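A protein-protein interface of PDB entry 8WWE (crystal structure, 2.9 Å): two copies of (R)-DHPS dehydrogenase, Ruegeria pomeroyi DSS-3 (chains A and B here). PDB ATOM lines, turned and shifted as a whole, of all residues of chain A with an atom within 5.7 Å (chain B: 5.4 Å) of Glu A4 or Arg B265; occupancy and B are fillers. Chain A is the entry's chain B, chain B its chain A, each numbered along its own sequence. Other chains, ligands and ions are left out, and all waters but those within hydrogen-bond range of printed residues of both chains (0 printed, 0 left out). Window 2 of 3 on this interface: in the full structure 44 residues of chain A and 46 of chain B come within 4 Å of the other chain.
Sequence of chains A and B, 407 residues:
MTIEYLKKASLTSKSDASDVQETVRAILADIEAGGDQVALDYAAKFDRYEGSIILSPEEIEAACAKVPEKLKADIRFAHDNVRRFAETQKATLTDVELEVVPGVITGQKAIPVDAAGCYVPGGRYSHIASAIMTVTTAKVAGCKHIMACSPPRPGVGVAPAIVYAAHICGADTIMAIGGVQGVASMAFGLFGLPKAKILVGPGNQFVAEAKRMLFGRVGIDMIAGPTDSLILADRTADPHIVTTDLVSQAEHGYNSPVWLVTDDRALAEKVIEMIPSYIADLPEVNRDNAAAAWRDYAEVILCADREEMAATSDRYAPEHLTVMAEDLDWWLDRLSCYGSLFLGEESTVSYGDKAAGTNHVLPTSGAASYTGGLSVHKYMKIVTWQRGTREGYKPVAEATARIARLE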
ATOM      1  N   THR A   2      12.765  -6.097  13.936  1.00  0.00           N
ATOM      2  CA  THR A   2      12.261  -4.887  13.319  1.00  0.00           C
ATOM      3  C   THR A   2      13.254  -3.763  13.718  1.00  0.00           C
ATOM      4  O   THR A   2      12.971  -2.581  13.609  1.00  0.00           O
ATOM      5  CB  THR A   2      10.859  -4.457  13.806  1.00  0.00           C
ATOM      6  OG1 THR A   2      11.006  -3.845  15.063  1.00  0.00           O
ATOM      7  CG2 THR A   2       9.982  -5.700  14.058  1.00  0.00           C
ATOM      8  N   ILE A   3      14.429  -4.212  14.252  1.00  0.00           N
ATOM      9  CA  ILE A   3      15.424  -3.397  14.944  1.00  0.00           C
ATOM     10  C   ILE A   3      16.316  -2.597  14.000  1.00  0.00           C
ATOM     11  O   ILE A   3      16.598  -3.018  12.874  1.00  0.00           O
ATOM     12  CB  ILE A   3      16.294  -4.314  15.831  1.00  0.00           C
ATOM     13  CG1 ILE A   3      16.922  -5.425  14.979  1.00  0.00           C
ATOM     14  CG2 ILE A   3      15.462  -4.925  16.923  1.00  0.00           C
ATOM     15  CD1 ILE A   3      18.064  -6.151  15.651  1.00  0.00           C
ATOM     16  N   GLU A   4      16.742  -1.407  14.457  1.00  0.00           N
ATOM     17  CA  GLU A   4      17.632  -0.516  13.714  1.00  0.00           C
ATOM     18  C   GLU A   4      18.855  -0.225  14.585  1.00  0.00           C
ATOM     19  O   GLU A   4      18.713   0.320  15.683  1.00  0.00           O
ATOM     20  CB  GLU A   4      16.892   0.772  13.313  1.00  0.00           C
ATOM     21  CG  GLU A   4      17.723   1.934  12.730  1.00  0.00           C
ATOM     22  CD  GLU A   4      16.887   3.232  12.582  1.00  0.00           C
ATOM     23  OE1 GLU A   4      17.464   4.355  12.613  1.00  0.00           O
ATOM     24  OE2 GLU A   4      15.644   3.138  12.441  1.00  0.00           O
ATOM     25  N   TYR A   5      20.061  -0.534  14.081  1.00  0.00           N
ATOM     26  CA  TYR A   5      21.308  -0.391  14.846  1.00  0.00           C
ATOM     27  C   TYR A   5      21.896   1.013  14.730  1.00  0.00           C
ATOM     28  O   TYR A   5      22.737   1.303  13.875  1.00  0.00           O
ATOM     29  CB  TYR A   5      22.313  -1.429  14.370  1.00  0.00           C
ATOM     30  CG  TYR A   5      22.186  -2.734  15.069  1.00  0.00           C
ATOM     31  CD1 TYR A   5      22.756  -2.913  16.309  1.00  0.00           C
ATOM     32  CD2 TYR A   5      21.478  -3.792  14.503  1.00  0.00           C
ATOM     33  CE1 TYR A   5      22.647  -4.100  16.976  1.00  0.00           C
ATOM     34  CE2 TYR A   5      21.363  -5.003  15.167  1.00  0.00           C
ATOM     35  CZ  TYR A   5      21.957  -5.140  16.415  1.00  0.00           C
ATOM     36  OH  TYR A   5      21.883  -6.291  17.155  1.00  0.00           O
ATOM     37  N   LEU A   6      21.523   1.859  15.687  1.00  0.00           N
ATOM     38  CA  LEU A   6      21.996   3.240  15.760  1.00  0.00           C
ATOM     39  C   LEU A   6      23.473   3.337  16.114  1.00  0.00           C
ATOM     40  O   LEU A   6      24.125   4.338  15.797  1.00  0.00           O
ATOM     41  CB  LEU A   6      21.161   3.939  16.826  1.00  0.00           C
ATOM     42  CG  LEU A   6      19.708   4.095  16.452  1.00  0.00           C
ATOM     43  CD1 LEU A   6      18.939   4.285  17.702  1.00  0.00           C
ATOM     44  CD2 LEU A   6      19.721   5.416  15.737  1.00  0.00           C
ATOM     45  N   THR B 262      16.203   0.898  23.275  1.00  0.00           N
ATOM     46  CA  THR B 262      15.197   1.926  23.487  1.00  0.00           C
ATOM     47  C   THR B 262      14.162   1.897  22.376  1.00  0.00           C
ATOM     48  O   THR B 262      14.404   1.350  21.306  1.00  0.00           O
ATOM     49  CB  THR B 262      15.891   3.304  23.615  1.00  0.00           C
ATOM     50  OG1 THR B 262      14.911   4.347  23.730  1.00  0.00           O
ATOM     51  CG2 THR B 262      16.886   3.578  22.481  1.00  0.00           C
ATOM     52  N   ASP B 263      12.988   2.489  22.643  1.00  0.00           N
ATOM     53  CA  ASP B 263      11.985   2.627  21.592  1.00  0.00           C
ATOM     54  C   ASP B 263      11.780   4.061  21.103  1.00  0.00           C
ATOM     55  O   ASP B 263      11.071   4.266  20.106  1.00  0.00           O
ATOM     56  CB  ASP B 263      10.639   2.016  22.022  1.00  0.00           C
ATOM     57  CG  ASP B 263       9.806   2.922  22.924  1.00  0.00           C
ATOM     58  OD1 ASP B 263      10.334   3.860  23.562  1.00  0.00           O
ATOM     59  OD2 ASP B 263       8.578   2.683  22.968  1.00  0.00           O
ATOM     60  N   ASP B 264      12.435   5.044  21.736  1.00  0.00           N
ATOM     61  CA  ASP B 264      12.323   6.456  21.380  1.00  0.00           C
ATOM     62  C   ASP B 264      13.628   6.840  20.706  1.00  0.00           C
ATOM     63  O   ASP B 264      14.656   6.980  21.378  1.00  0.00           O
ATOM     64  CB  ASP B 264      12.057   7.312  22.615  1.00  0.00           C
ATOM     65  CG  ASP B 264      12.377   8.795  22.400  1.00  0.00           C
ATOM     66  OD1 ASP B 264      11.736   9.452  21.547  1.00  0.00           O
ATOM     67  OD2 ASP B 264      13.295   9.284  23.100  1.00  0.00           O
ATOM     68  N   ARG B 265      13.574   7.018  19.376  1.00  0.00           N
ATOM     69  CA  ARG B 265      14.756   7.345  18.574  1.00  0.00           C
ATOM     70  C   ARG B 265      15.531   8.536  19.134  1.00  0.00           C
ATOM     71  O   ARG B 265      16.779   8.517  19.212  1.00  0.00           O
ATOM     72  CB  ARG B 265      14.291   7.597  17.130  1.00  0.00           C
ATOM     73  CG  ARG B 265      15.389   7.784  16.067  1.00  0.00           C
ATOM     74  CD  ARG B 265      14.834   8.551  14.862  1.00  0.00           C
ATOM     75  NE  ARG B 265      13.485   8.121  14.462  1.00  0.00           N
ATOM     76  CZ  ARG B 265      13.195   7.014  13.768  1.00  0.00           C
ATOM     77  NH1 ARG B 265      14.157   6.177  13.380  1.00  0.00           N
ATOM     78  NH2 ARG B 265      11.927   6.740  13.463  1.00  0.00           N
ATOM     79  N   ALA B 266      14.794   9.568  19.551  1.00  0.00           N
ATOM     80  CA  ALA B 266      15.393  10.819  19.996  1.00  0.00           C
ATOM     81  C   ALA B 266      16.438  10.576  21.069  1.00  0.00           C
ATOM     82  O   ALA B 266      17.571  11.074  20.970  1.00  0.00           O
ATOM     83  CB  ALA B 266      14.313  11.777  20.498  1.00  0.00           C
ATOM     84  N   LEU B 267      16.052   9.848  22.125  1.00  0.00           N
ATOM     85  CA  LEU B 267      16.958   9.556  23.237  1.00  0.00           C
ATOM     86  C   LEU B 267      18.261   8.941  22.755  1.00  0.00           C
ATOM     87  O   LEU B 267      19.348   9.328  23.203  1.00  0.00           O
ATOM     88  CB  LEU B 267      16.280   8.638  24.255  1.00  0.00           C
ATOM     89  CG  LEU B 267      17.244   8.309  25.398  1.00  0.00           C
ATOM     90  CD1 LEU B 267      17.555   9.571  26.183  1.00  0.00           C
ATOM     91  CD2 LEU B 267      16.684   7.227  26.300  1.00  0.00           C
ATOM     92  N   ALA B 268      18.159   7.897  21.941  1.00  0.00           N
ATOM     93  CA  ALA B 268      19.351   7.220  21.456  1.00  0.00           C
ATOM     94  C   ALA B 268      20.332   8.223  20.855  1.00  0.00           C
ATOM     95  O   ALA B 268      21.505   8.277  21.255  1.00  0.00           O
ATOM     96  CB  ALA B 268      18.979   6.137  20.450  1.00  0.00           C
ATOM     97  N   GLU B 269      19.857   9.038  19.894  1.00  0.00           N
ATOM     98  CA  GLU B 269      20.759   9.978  19.224  1.00  0.00           C
ATOM     99  C   GLU B 269      21.328  10.982  20.229  1.00  0.00           C
ATOM    100  O   GLU B 269      22.524  11.330  20.193  1.00  0.00           O
ATOM    101  CB  GLU B 269      20.037  10.687  18.082  1.00  0.00           C
ATOM    102  CG  GLU B 269      19.788   9.827  16.830  1.00  0.00           C
ATOM    103  CD  GLU B 269      18.468  10.171  16.120  1.00  0.00           C
ATOM    104  OE1 GLU B 269      17.862  11.206  16.494  1.00  0.00           O
ATOM    105  OE2 GLU B 269      18.043   9.424  15.196  1.00  0.00           O
ATOM    106  N   LYS B 270      20.475  11.432  21.159  1.00  0.00           N
ATOM    107  CA  LYS B 270      20.854  12.418  22.163  1.00  0.00           C
ATOM    108  C   LYS B 270      22.043  11.920  22.987  1.00  0.00           C
ATOM    109  O   LYS B 270      23.057  12.618  23.141  1.00  0.00           O
ATOM    110  CB  LYS B 270      19.609  12.670  23.017  1.00  0.00           C
ATOM    111  CG  LYS B 270      19.645  13.773  24.060  1.00  0.00           C
ATOM    112  CD  LYS B 270      18.218  14.082  24.540  1.00  0.00           C
ATOM    113  CE  LYS B 270      18.154  15.435  25.235  1.00  0.00           C
ATOM    114  NZ  LYS B 270      18.017  15.375  26.725  1.00  0.00           N
ATOM    115  N   VAL B 300      23.766   0.602  20.464  1.00  0.00           N
ATOM    116  CA  VAL B 300      22.487   1.276  20.642  1.00  0.00           C
ATOM    117  C   VAL B 300      21.491   0.704  19.633  1.00  0.00           C
ATOM    118  O   VAL B 300      21.765   0.674  18.429  1.00  0.00           O
ATOM    119  CB  VAL B 300      22.615   2.799  20.486  1.00  0.00           C
ATOM    120  CG1 VAL B 300      21.305   3.414  20.779  1.00  0.00           C
ATOM    121  CG2 VAL B 300      23.639   3.328  21.422  1.00  0.00           C
ATOM    122  N   ILE B 301      20.349   0.219  20.125  1.00  0.00           N
ATOM    123  CA  ILE B 301      19.404  -0.523  19.305  1.00  0.00           C
ATOM    124  C   ILE B 301      18.049   0.140  19.436  1.00  0.00           C
ATOM    125  O   ILE B 301      17.491   0.218  20.545  1.00  0.00           O
ATOM    126  CB  ILE B 301      19.343  -2.004  19.718  1.00  0.00           C
ATOM    127  CG1 ILE B 301      20.689  -2.649  19.406  1.00  0.00           C
ATOM    128  CG2 ILE B 301      18.235  -2.757  19.027  1.00  0.00           C
ATOM    129  CD1 ILE B 301      20.900  -3.919  20.114  1.00  0.00           C
ATOM    130  N   LEU B 302      17.486   0.543  18.289  1.00  0.00           N
ATOM    131  CA  LEU B 302      16.215   1.247  18.218  1.00  0.00           C
ATOM    132  C   LEU B 302      15.074   0.295  17.969  1.00  0.00           C
ATOM    133  O   LEU B 302      15.082  -0.483  17.008  1.00  0.00           O
ATOM    134  CB  LEU B 302      16.203   2.298  17.118  1.00  0.00           C
ATOM    135  CG  LEU B 302      14.926   3.116  17.310  1.00  0.00           C
ATOM    136  CD1 LEU B 302      14.680   3.549  18.788  1.00  0.00           C
ATOM    137  CD2 LEU B 302      14.948   4.289  16.378  1.00  0.00           C
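NH1 of Arg B265 is in salt-bridge range of OE2 of Glu A4, at 3.5 Å.
N of Leu A6 sits at hydrogen-bond distance from O of Val B300 (3.0 Å).
The backbone NH (N) of Leu B302 sits at hydrogen-bond distance from the backbone carbonyl oxygen (O) of Glu A4, at 2.9 Å.
The backbone carbonyl oxygen of Ile B301 lies within hydrogen-bond range of the backbone NH of Thr B262 (3.1 Å).
O of Leu B302 touches CA of Ile A3, 3.6 Å away.
O of Glu A4 touches CA of Ile B301 (3.8 Å).
C of Tyr A5 touches O of Val B300 (3.7 Å).
Ile B301 touches Tyr A5 (CG1 to CE1, 3.4 Å).
Ala B268 touches Leu A6.
Leu A6 touches Leu B302 (CD1 to CB, 3.4 Å).
Of the printed residues of chain B, Ile A3 touches Leu B302 (3.6 Å).
Glu A4 touches just these residues of chain B: Arg B265 (3.5 Å), Ile B301 (3.8 Å) and Leu B302 (2.9 Å).
Of the printed residues of chain B, Leu A6 touches Ala B268 (3.3 Å), Val B300 (3.0 Å) and Leu B302 (3.4 Å).
Thr B262 touches none of the printed residues of chain A.
Arg B265 touches just one residue of chain A: Glu A4 (3.5 Å).
The nearest residue of chain A that does not touch Arg B265 is Leu A6 (4.9 Å).
The nearest printed residue of chain A that does not touch Ala B268 is Glu A4 (7.5 Å).
Printed residues of chain A that touch a printed residue of chain B: Ile A3, Glu A4, Tyr A5 and Leu A6.
Of the 12 printed residues of chain B, 5 touch a printed residue of chain A.
Printed residues of chain B that touch a printed residue of chain A: Arg B265, Ala B268, Val B300, Ile B301 and Leu B302.
No position is printed for both chains.
Of the 9 pairs that touch across the chains among the printed residues, none has its exchanged pair printed and touching as well.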
